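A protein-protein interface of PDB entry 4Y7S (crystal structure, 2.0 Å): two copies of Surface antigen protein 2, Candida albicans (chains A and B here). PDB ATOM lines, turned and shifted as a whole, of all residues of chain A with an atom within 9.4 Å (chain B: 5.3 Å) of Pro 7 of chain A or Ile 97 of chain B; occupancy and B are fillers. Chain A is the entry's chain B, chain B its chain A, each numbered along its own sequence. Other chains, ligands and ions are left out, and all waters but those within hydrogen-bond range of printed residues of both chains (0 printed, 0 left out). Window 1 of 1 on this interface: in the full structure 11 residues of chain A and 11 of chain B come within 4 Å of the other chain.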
ATOM      1  N   PRO A   2      -7.002  16.170  25.095  1.00  0.00           N
ATOM      2  CA  PRO A   2      -6.999  14.749  25.488  1.00  0.00           C
ATOM      3  C   PRO A   2      -7.891  13.811  24.659  1.00  0.00           C
ATOM      4  O   PRO A   2      -7.683  12.604  24.682  1.00  0.00           O
ATOM      5  CB  PRO A   2      -7.476  14.795  26.950  1.00  0.00           C
ATOM      6  CG  PRO A   2      -8.164  16.077  27.116  1.00  0.00           C
ATOM      7  CD  PRO A   2      -7.558  17.042  26.146  1.00  0.00           C
ATOM      8  N   TYR A   3      -8.810  14.359  23.876  1.00  0.00           N
ATOM      9  CA  TYR A   3      -9.830  13.557  23.196  1.00  0.00           C
ATOM     10  C   TYR A   3      -9.497  13.159  21.749  1.00  0.00           C
ATOM     11  O   TYR A   3     -10.366  12.657  21.041  1.00  0.00           O
ATOM     12  CB  TYR A   3     -11.156  14.301  23.258  1.00  0.00           C
ATOM     13  CG  TYR A   3     -11.636  14.480  24.682  1.00  0.00           C
ATOM     14  CD1 TYR A   3     -12.269  13.438  25.354  1.00  0.00           C
ATOM     15  CD2 TYR A   3     -11.398  15.660  25.380  1.00  0.00           C
ATOM     16  CE1 TYR A   3     -12.712  13.593  26.663  1.00  0.00           C
ATOM     17  CE2 TYR A   3     -11.821  15.814  26.685  1.00  0.00           C
ATOM     18  CZ  TYR A   3     -12.469  14.773  27.323  1.00  0.00           C
ATOM     19  OH  TYR A   3     -12.881  14.918  28.624  1.00  0.00           O
ATOM     20  N   THR A   4      -8.257  13.369  21.303  1.00  0.00           N
ATOM     21  CA  THR A   4      -7.905  13.059  19.912  1.00  0.00           C
ATOM     22  C   THR A   4      -7.744  11.547  19.711  1.00  0.00           C
ATOM     23  O   THR A   4      -7.595  11.088  18.586  1.00  0.00           O
ATOM     24  CB  THR A   4      -6.594  13.746  19.472  1.00  0.00           C
ATOM     25  OG1 THR A   4      -5.481  13.165  20.158  1.00  0.00           O
ATOM     26  CG2 THR A   4      -6.657  15.264  19.718  1.00  0.00           C
ATOM     27  N   ILE A   5      -7.810  10.775  20.794  1.00  0.00           N
ATOM     28  CA  ILE A   5      -7.803   9.312  20.709  1.00  0.00           C
ATOM     29  C   ILE A   5      -9.184   8.754  20.334  1.00  0.00           C
ATOM     30  O   ILE A   5      -9.381   7.540  20.283  1.00  0.00           O
ATOM     31  CB  ILE A   5      -7.328   8.659  22.036  1.00  0.00           C
ATOM     32  CG1 ILE A   5      -8.303   8.968  23.184  1.00  0.00           C
ATOM     33  CG2 ILE A   5      -5.964   9.165  22.398  1.00  0.00           C
ATOM     34  CD1 ILE A   5      -8.127   8.067  24.405  1.00  0.00           C
ATOM     35  N   TYR A   6     -10.155   9.642  20.168  1.00  0.00           N
ATOM     36  CA  TYR A   6     -11.499   9.263  19.739  1.00  0.00           C
ATOM     37  C   TYR A   6     -11.687   9.703  18.298  1.00  0.00           C
ATOM     38  O   TYR A   6     -10.935  10.572  17.812  1.00  0.00           O
ATOM     39  CB  TYR A   6     -12.551   9.888  20.656  1.00  0.00           C
ATOM     40  CG  TYR A   6     -12.381   9.397  22.079  1.00  0.00           C
ATOM     41  CD1 TYR A   6     -12.610   8.068  22.405  1.00  0.00           C
ATOM     42  CD2 TYR A   6     -11.929  10.246  23.079  1.00  0.00           C
ATOM     43  CE1 TYR A   6     -12.428   7.595  23.720  1.00  0.00           C
ATOM     44  CE2 TYR A   6     -11.741   9.789  24.383  1.00  0.00           C
ATOM     45  CZ  TYR A   6     -11.992   8.455  24.693  1.00  0.00           C
ATOM     46  OH  TYR A   6     -11.810   7.978  25.975  1.00  0.00           O
ATOM     47  N   PRO A   7     -12.664   9.095  17.595  1.00  0.00           N
ATOM     48  CA  PRO A   7     -13.050   9.571  16.262  1.00  0.00           C
ATOM     49  C   PRO A   7     -13.495  11.026  16.346  1.00  0.00           C
ATOM     50  O   PRO A   7     -14.195  11.369  17.297  1.00  0.00           O
ATOM     51  CB  PRO A   7     -14.238   8.675  15.880  1.00  0.00           C
ATOM     52  CG  PRO A   7     -14.058   7.453  16.703  1.00  0.00           C
ATOM     53  CD  PRO A   7     -13.445   7.907  17.992  1.00  0.00           C
ATOM     54  N   PRO A   8     -13.097  11.864  15.388  1.00  0.00           N
ATOM     55  CA  PRO A   8     -13.491  13.275  15.416  1.00  0.00           C
ATOM     56  C   PRO A   8     -14.984  13.491  15.256  1.00  0.00           C
ATOM     57  O   PRO A   8     -15.663  12.657  14.666  1.00  0.00           O
ATOM     58  CB  PRO A   8     -12.742  13.875  14.228  1.00  0.00           C
ATOM     59  CG  PRO A   8     -12.505  12.737  13.311  1.00  0.00           C
ATOM     60  CD  PRO A   8     -12.338  11.522  14.176  1.00  0.00           C
ATOM     61  N   VAL A   9     -15.478  14.587  15.817  1.00  0.00           N
ATOM     62  CA  VAL A   9     -16.870  14.988  15.669  1.00  0.00           C
ATOM     63  C   VAL A   9     -16.920  16.446  15.233  1.00  0.00           C
ATOM     64  O   VAL A   9     -16.028  17.228  15.570  1.00  0.00           O
ATOM     65  CB  VAL A   9     -17.674  14.825  16.982  1.00  0.00           C
ATOM     66  CG1 VAL A   9     -17.890  13.375  17.294  1.00  0.00           C
ATOM     67  CG2 VAL A   9     -16.962  15.546  18.125  1.00  0.00           C
ATOM     68  N   PRO A  10     -17.962  16.826  14.544  1.00  0.00           N
ATOM     69  CA  PRO A  10     -18.170  18.215  14.173  1.00  0.00           C
ATOM     70  C   PRO A  10     -18.263  19.077  15.408  1.00  0.00           C
ATOM     71  O   PRO A  10     -18.859  18.698  16.368  1.00  0.00           O
ATOM     72  CB  PRO A  10     -19.496  18.165  13.433  1.00  0.00           C
ATOM     73  CG  PRO A  10     -19.536  16.802  12.878  1.00  0.00           C
ATOM     74  CD  PRO A  10     -18.993  15.973  13.992  1.00  0.00           C
ATOM     75  N   LYS A  11     -17.636  20.218  15.376  1.00  0.00           N
ATOM     76  CA  LYS A  11     -17.630  21.125  16.480  1.00  0.00           C
ATOM     77  C   LYS A  11     -18.765  22.131  16.476  1.00  0.00           C
ATOM     78  O   LYS A  11     -18.694  23.142  17.137  1.00  0.00           O
ATOM     79  CB  LYS A  11     -16.373  21.930  16.444  1.00  0.00           C
ATOM     80  CG  LYS A  11     -15.109  21.110  16.424  1.00  0.00           C
ATOM     81  CD  LYS A  11     -14.885  20.476  17.761  1.00  0.00           C
ATOM     82  CE  LYS A  11     -13.514  19.841  17.814  1.00  0.00           C
ATOM     83  NZ  LYS A  11     -12.456  20.858  18.079  1.00  0.00           N
ATOM     84  N   ARG A  21     -26.544  12.866  15.194  1.00  0.00           N
ATOM     85  CA  ARG A  21     -26.088  11.616  14.578  1.00  0.00           C
ATOM     86  C   ARG A  21     -27.235  10.747  14.121  1.00  0.00           C
ATOM     87  O   ARG A  21     -27.052   9.902  13.257  1.00  0.00           O
ATOM     88  CB  ARG A  21     -25.213  10.810  15.530  1.00  0.00           C
ATOM     89  CG  ARG A  21     -23.994  11.554  15.980  1.00  0.00           C
ATOM     90  CD  ARG A  21     -23.038  11.937  14.834  1.00  0.00           C
ATOM     91  NE  ARG A  21     -22.188  12.998  15.353  1.00  0.00           N
ATOM     92  CZ  ARG A  21     -22.371  14.295  15.119  1.00  0.00           C
ATOM     93  NH1 ARG A  21     -23.326  14.719  14.308  1.00  0.00           N
ATOM     94  NH2 ARG A  21     -21.566  15.179  15.683  1.00  0.00           N
ATOM     95  N   TRP A  46     -21.888  19.856  21.236  1.00  0.00           N
ATOM     96  CA  TRP A  46     -21.634  19.086  20.017  1.00  0.00           C
ATOM     97  C   TRP A  46     -20.973  17.732  20.275  1.00  0.00           C
ATOM     98  O   TRP A  46     -20.726  16.959  19.346  1.00  0.00           O
ATOM     99  CB  TRP A  46     -20.761  19.892  19.052  1.00  0.00           C
ATOM    100  CG  TRP A  46     -19.585  20.573  19.695  1.00  0.00           C
ATOM    101  CD1 TRP A  46     -19.481  21.901  20.003  1.00  0.00           C
ATOM    102  CD2 TRP A  46     -18.357  19.968  20.113  1.00  0.00           C
ATOM    103  NE1 TRP A  46     -18.264  22.156  20.582  1.00  0.00           N
ATOM    104  CE2 TRP A  46     -17.553  20.989  20.660  1.00  0.00           C
ATOM    105  CE3 TRP A  46     -17.855  18.666  20.074  1.00  0.00           C
ATOM    106  CZ2 TRP A  46     -16.283  20.747  21.167  1.00  0.00           C
ATOM    107  CZ3 TRP A  46     -16.597  18.426  20.581  1.00  0.00           C
ATOM    108  CH2 TRP A  46     -15.821  19.462  21.119  1.00  0.00           C
ATOM    109  N   ASP A  47     -20.681  17.451  21.535  1.00  0.00           N
ATOM    110  CA  ASP A  47     -19.892  16.286  21.913  1.00  0.00           C
ATOM    111  C   ASP A  47     -20.723  15.024  22.131  1.00  0.00           C
ATOM    112  O   ASP A  47     -21.192  14.759  23.246  1.00  0.00           O
ATOM    113  CB  ASP A  47     -19.133  16.614  23.191  1.00  0.00           C
ATOM    114  CG  ASP A  47     -18.179  15.532  23.608  1.00  0.00           C
ATOM    115  OD1 ASP A  47     -18.178  14.402  23.069  1.00  0.00           O
ATOM    116  OD2 ASP A  47     -17.436  15.830  24.550  1.00  0.00           O
ATOM    117  N   THR A  48     -20.851  14.227  21.079  1.00  0.00           N
ATOM    118  CA  THR A  48     -21.606  12.974  21.102  1.00  0.00           C
ATOM    119  C   THR A  48     -21.225  12.021  22.247  1.00  0.00           C
ATOM    120  O   THR A  48     -22.080  11.565  23.001  1.00  0.00           O
ATOM    121  CB  THR A  48     -21.406  12.218  19.768  1.00  0.00           C
ATOM    122  OG1 THR A  48     -21.717  13.093  18.675  1.00  0.00           O
ATOM    123  CG2 THR A  48     -22.287  10.980  19.714  1.00  0.00           C
ATOM    124  N   GLY A  49     -19.941  11.704  22.341  1.00  0.00           N
ATOM    125  CA  GLY A  49     -19.438  10.789  23.341  1.00  0.00           C
ATOM    126  C   GLY A  49     -19.796  11.213  24.755  1.00  0.00           C
ATOM    127  O   GLY A  49     -20.246  10.406  25.560  1.00  0.00           O
ATOM    128  N   ALA A  84     -24.668   4.996  17.569  1.00  0.00           N
ATOM    129  CA  ALA A  84     -24.005   6.286  17.487  1.00  0.00           C
ATOM    130  C   ALA A  84     -22.989   6.457  18.605  1.00  0.00           C
ATOM    131  O   ALA A  84     -21.891   6.970  18.394  1.00  0.00           O
ATOM    132  CB  ALA A  84     -25.016   7.405  17.535  1.00  0.00           C
ATOM    133  N   CYS A  85     -23.362   6.044  19.805  1.00  0.00           N
ATOM    134  CA  CYS A  85     -22.480   6.215  20.936  1.00  0.00           C
ATOM    135  C   CYS A  85     -21.279   5.316  20.801  1.00  0.00           C
ATOM    136  O   CYS A  85     -20.150   5.722  21.091  1.00  0.00           O
ATOM    137  CB  CYS A  85     -23.223   5.954  22.239  1.00  0.00           C
ATOM    138  SG  CYS A  85     -24.517   7.162  22.539  1.00  0.00           S
ATOM    139  N   ALA A  86     -21.510   4.100  20.327  1.00  0.00           N
ATOM    140  CA  ALA A  86     -20.411   3.174  20.096  1.00  0.00           C
ATOM    141  C   ALA A  86     -19.460   3.735  19.046  1.00  0.00           C
ATOM    142  O   ALA A  86     -18.236   3.665  19.195  1.00  0.00           O
ATOM    143  CB  ALA A  86     -20.935   1.799  19.666  1.00  0.00           C
ATOM    144  N   ALA A  87     -20.010   4.297  17.978  1.00  0.00           N
ATOM    145  CA  ALA A  87     -19.150   4.827  16.921  1.00  0.00           C
ATOM    146  C   ALA A  87     -18.353   6.041  17.407  1.00  0.00           C
ATOM    147  O   ALA A  87     -17.286   6.349  16.881  1.00  0.00           O
ATOM    148  CB  ALA A  87     -19.945   5.185  15.725  1.00  0.00           C
ATOM    149  N   ALA A  88     -18.870   6.731  18.404  1.00  0.00           N
ATOM    150  CA  ALA A  88     -18.176   7.882  18.944  1.00  0.00           C
ATOM    151  C   ALA A  88     -17.005   7.462  19.834  1.00  0.00           C
ATOM    152  O   ALA A  88     -16.130   8.278  20.122  1.00  0.00           O
ATOM    153  CB  ALA A  88     -19.144   8.762  19.733  1.00  0.00           C
ATOM    154  N   GLY A  89     -16.974   6.190  20.224  1.00  0.00           N
ATOM    155  CA  GLY A  89     -15.866   5.636  20.989  1.00  0.00           C
ATOM    156  C   GLY A  89     -16.173   5.354  22.453  1.00  0.00           C
ATOM    157  O   GLY A  89     -15.267   5.077  23.246  1.00  0.00           O
ATOM    158  N   VAL A  90     -17.449   5.399  22.817  1.00  0.00           N
ATOM    159  CA  VAL A  90     -17.857   5.132  24.199  1.00  0.00           C
ATOM    160  C   VAL A  90     -17.681   3.655  24.521  1.00  0.00           C
ATOM    161  O   VAL A  90     -17.766   2.809  23.643  1.00  0.00           O
ATOM    162  CB  VAL A  90     -19.326   5.542  24.425  1.00  0.00           C
ATOM    163  CG1 VAL A  90     -19.765   5.317  25.856  1.00  0.00           C
ATOM    164  CG2 VAL A  90     -19.501   6.975  24.065  1.00  0.00           C
ATOM    165  N   PRO B  55     -14.408   2.090  17.048  1.00  0.00           N
ATOM    166  CA  PRO B  55     -13.019   2.558  17.002  1.00  0.00           C
ATOM    167  C   PRO B  55     -12.017   1.683  17.732  1.00  0.00           C
ATOM    168  O   PRO B  55     -10.856   1.710  17.348  1.00  0.00           O
ATOM    169  CB  PRO B  55     -13.089   3.954  17.635  1.00  0.00           C
ATOM    170  CG  PRO B  55     -14.365   4.020  18.339  1.00  0.00           C
ATOM    171  CD  PRO B  55     -15.305   3.106  17.629  1.00  0.00           C
ATOM    172  N   THR B  58     -11.344  -0.537  14.632  1.00  0.00           N
ATOM    173  CA  THR B  58     -10.713   0.134  13.497  1.00  0.00           C
ATOM    174  C   THR B  58      -9.372   0.741  13.899  1.00  0.00           C
ATOM    175  O   THR B  58      -8.463   0.825  13.088  1.00  0.00           O
ATOM    176  CB  THR B  58     -11.590   1.248  12.912  1.00  0.00           C
ATOM    177  OG1 THR B  58     -11.712   2.302  13.863  1.00  0.00           O
ATOM    178  CG2 THR B  58     -12.971   0.716  12.517  1.00  0.00           C
ATOM    179  N   GLY B  59      -9.274   1.207  15.136  1.00  0.00           N
ATOM    180  CA  GLY B  59      -8.050   1.836  15.619  1.00  0.00           C
ATOM    181  C   GLY B  59      -6.927   0.818  15.740  1.00  0.00           C
ATOM    182  O   GLY B  59      -5.763   1.106  15.460  1.00  0.00           O
ATOM    183  N   ARG B  78      -6.123   2.402   2.863  1.00  0.00           N
ATOM    184  CA  ARG B  78      -7.193   3.267   3.330  1.00  0.00           C
ATOM    185  C   ARG B  78      -8.304   3.404   2.274  1.00  0.00           C
ATOM    186  O   ARG B  78      -9.480   3.450   2.624  1.00  0.00           O
ATOM    187  CB  ARG B  78      -6.689   4.661   3.695  1.00  0.00           C
ATOM    188  CG  ARG B  78      -5.812   4.713   4.914  1.00  0.00           C
ATOM    189  CD  ARG B  78      -5.514   6.172   5.336  1.00  0.00           C
ATOM    190  NE  ARG B  78      -6.561   6.763   6.184  1.00  0.00           N
ATOM    191  CZ  ARG B  78      -6.429   7.914   6.850  1.00  0.00           C
ATOM    192  NH1 ARG B  78      -5.306   8.614   6.760  1.00  0.00           N
ATOM    193  NH2 ARG B  78      -7.424   8.374   7.592  1.00  0.00           N
ATOM    194  N   TRP B  95     -14.786   4.676   6.984  1.00  0.00           N
ATOM    195  CA  TRP B  95     -13.955   3.872   7.873  1.00  0.00           C
ATOM    196  C   TRP B  95     -13.645   4.747   9.085  1.00  0.00           C
ATOM    197  O   TRP B  95     -12.844   5.669   9.006  1.00  0.00           O
ATOM    198  CB  TRP B  95     -12.699   3.379   7.163  1.00  0.00           C
ATOM    199  CG  TRP B  95     -11.871   2.423   7.985  1.00  0.00           C
ATOM    200  CD1 TRP B  95     -12.314   1.311   8.638  1.00  0.00           C
ATOM    201  CD2 TRP B  95     -10.464   2.491   8.222  1.00  0.00           C
ATOM    202  NE1 TRP B  95     -11.281   0.696   9.281  1.00  0.00           N
ATOM    203  CE2 TRP B  95     -10.126   1.392   9.037  1.00  0.00           C
ATOM    204  CE3 TRP B  95      -9.448   3.373   7.825  1.00  0.00           C
ATOM    205  CZ2 TRP B  95      -8.829   1.158   9.469  1.00  0.00           C
ATOM    206  CZ3 TRP B  95      -8.160   3.133   8.252  1.00  0.00           C
ATOM    207  CH2 TRP B  95      -7.858   2.029   9.058  1.00  0.00           C
ATOM    208  N   ILE B  96     -14.327   4.490  10.195  1.00  0.00           N
ATOM    209  CA  ILE B  96     -14.330   5.440  11.303  1.00  0.00           C
ATOM    210  C   ILE B  96     -13.218   5.139  12.289  1.00  0.00           C
ATOM    211  O   ILE B  96     -13.356   4.259  13.127  1.00  0.00           O
ATOM    212  CB  ILE B  96     -15.665   5.408  12.096  1.00  0.00           C
ATOM    213  CG1 ILE B  96     -16.901   5.427  11.173  1.00  0.00           C
ATOM    214  CG2 ILE B  96     -15.713   6.557  13.091  1.00  0.00           C
ATOM    215  CD1 ILE B  96     -17.139   6.707  10.418  1.00  0.00           C
ATOM    216  N   ILE B  97     -12.147   5.925  12.235  1.00  0.00           N
ATOM    217  CA  ILE B  97     -10.986   5.697  13.096  1.00  0.00           C
ATOM    218  C   ILE B  97     -10.730   6.871  14.009  1.00  0.00           C
ATOM    219  O   ILE B  97     -11.120   7.999  13.710  1.00  0.00           O
ATOM    220  CB  ILE B  97      -9.703   5.422  12.265  1.00  0.00           C
ATOM    221  CG1 ILE B  97      -9.445   6.529  11.238  1.00  0.00           C
ATOM    222  CG2 ILE B  97      -9.810   4.107  11.588  1.00  0.00           C
ATOM    223  CD1 ILE B  97      -8.128   6.351  10.450  1.00  0.00           C
ATOM    224  N   PRO B  98     -10.040   6.619  15.125  1.00  0.00           N
ATOM    225  CA  PRO B  98      -9.632   7.717  16.000  1.00  0.00           C
ATOM    226  C   PRO B  98      -8.764   8.770  15.266  1.00  0.00           C
ATOM    227  O   PRO B  98      -8.041   8.424  14.324  1.00  0.00           O
ATOM    228  CB  PRO B  98      -8.804   7.014  17.059  1.00  0.00           C
ATOM    229  CG  PRO B  98      -9.257   5.586  17.034  1.00  0.00           C
ATOM    230  CD  PRO B  98      -9.587   5.309  15.627  1.00  0.00           C
ATOM    231  N   ALA B  99      -8.836  10.028  15.680  1.00  0.00           N
ATOM    232  CA  ALA B  99      -8.042  11.071  15.041  1.00  0.00           C
ATOM    233  C   ALA B  99      -6.541  10.799  15.172  1.00  0.00           C
ATOM    234  O   ALA B  99      -5.783  11.055  14.246  1.00  0.00           O
ATOM    235  CB  ALA B  99      -8.378  12.435  15.615  1.00  0.00           C
ATOM    236  N   VAL B 101      -5.077   7.897  15.285  1.00  0.00           N
ATOM    237  CA  VAL B 101      -4.739   6.834  14.336  1.00  0.00           C
ATOM    238  C   VAL B 101      -4.676   7.362  12.903  1.00  0.00           C
ATOM    239  O   VAL B 101      -3.775   6.997  12.131  1.00  0.00           O
ATOM    240  CB  VAL B 101      -5.751   5.669  14.414  1.00  0.00           C
ATOM    241  CG1 VAL B 101      -5.499   4.650  13.303  1.00  0.00           C
ATOM    242  CG2 VAL B 101      -5.699   5.003  15.798  1.00  0.00           C
ATOM    243  N   SER B 102      -5.616   8.224  12.535  1.00  0.00           N
ATOM    244  CA  SER B 102      -5.562   8.865  11.225  1.00  0.00           C
ATOM    245  C   SER B 102      -4.243   9.619  11.037  1.00  0.00           C
ATOM    246  O   SER B 102      -3.647   9.544   9.975  1.00  0.00           O
ATOM    247  CB  SER B 102      -6.736   9.825  11.034  1.00  0.00           C
ATOM    248  OG  SER B 102      -6.837  10.206   9.669  1.00  0.00           O
ATOM    249  N   LEU B 105      -1.503   7.260  10.378  1.00  0.00           N
ATOM    250  CA  LEU B 105      -1.559   6.733   9.018  1.00  0.00           C
ATOM    251  C   LEU B 105      -1.047   7.751   8.024  1.00  0.00           C
ATOM    252  O   LEU B 105      -0.301   7.404   7.108  1.00  0.00           O
ATOM    253  CB  LEU B 105      -2.978   6.324   8.649  1.00  0.00           C
ATOM    254  CG  LEU B 105      -3.482   5.051   9.334  1.00  0.00           C
ATOM    255  CD1 LEU B 105      -4.988   4.923   9.170  1.00  0.00           C
ATOM    256  CD2 LEU B 105      -2.730   3.809   8.808  1.00  0.00           C
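Of the 12 printed residues of chain B, 5 touch a printed residue of chain A.
Hydrophobic or aromatic side chains of chain B that line the printed part of chain A: Pro 55, Ile 96, Pro 98 and Ala 99.
Of the 22 printed residues of chain A, 8 touch a printed residue of chain B.
Among the printed residues, 12 pairs touch across the chains.
Among the printed residues, no Asp or Glu carboxylate lies within 4 Å of a Lys or Arg side-chain nitrogen of the other chain.
Of chain A, only Pro 7 and Pro 8 come within 4 Å of Ile 97 of chain B.
Pro 98 of chain B touches just these residues of chain A: Ile 5 (3.3 Å), Tyr 6 (3.6 Å) and Pro 7 (3.7 Å).
Of the printed residues of chain B, Gly 89 of chain A touches Pro 55 (3.4 Å).
Of the printed residues of chain B, Ala 87 of chain A touches Pro 55.
Of the printed residues of chain B, Pro 8 of chain A touches Ile 97.
Of the printed residues of chain A, Ile 96 of chain B touches Pro 7 (3.8 Å).
Of the printed residues of chain A, Ala 99 of chain B touches Thr 4 (3.3 Å) and Tyr 6 (3.0 Å).
Cys 85 of chain A touches none of the printed residues of chain B.
The nearest residue of chain B that does not touch Pro 7 of chain A is Ala 99 of chain B (4.3 Å).
The nearest residue of chain A that does not touch Ile 97 of chain B is Tyr 6 of chain A (4.8 Å).
The backbone carbonyl oxygen of Ile 96 of chain B is in hydrogen-bond range of the side-chain hydroxyl of Thr 58 of chain B (2.7 Å).
Pro 98 of chain B touches Ile 5 of chain A (CB to O, 3.3 Å).
Tyr 6 of chain A touches Pro 98 of chain B.
Pro 7 of chain A touches Pro 55 of chain B.
Pro 7 of chain A touches Ile 96 of chain B.
Pro 7 of chain A touches Ile 97 of chain B.
Pro 7 of chain A touches Pro 98 of chain B.
O of Ile 97 of chain B touches CD of Pro 8 of chain A, at 3.8 Å.
Pro 55 of chain B touches Ala 86 of chain A (CD to O, 3.4 Å).
Ala 87 of chain A touches Pro 55 of chain B.
CG of Pro 55 of chain B touches CA of Gly 89 of chain A (3.4 Å).
No position is printed for both chains.
Of the 12 pairs that touch across the chains among the printed residues, none has its exchanged pair printed and touching as well.
The backbone NH (N) of Ala 99 of chain B lies within hydrogen-bond range of the backbone carbonyl oxygen (O) of Thr 4 of chain A, 3.3 Å away.
N of Ala 99 of chain B sits at hydrogen-bond distance from O of Tyr 6 of chain A (3.0 Å).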
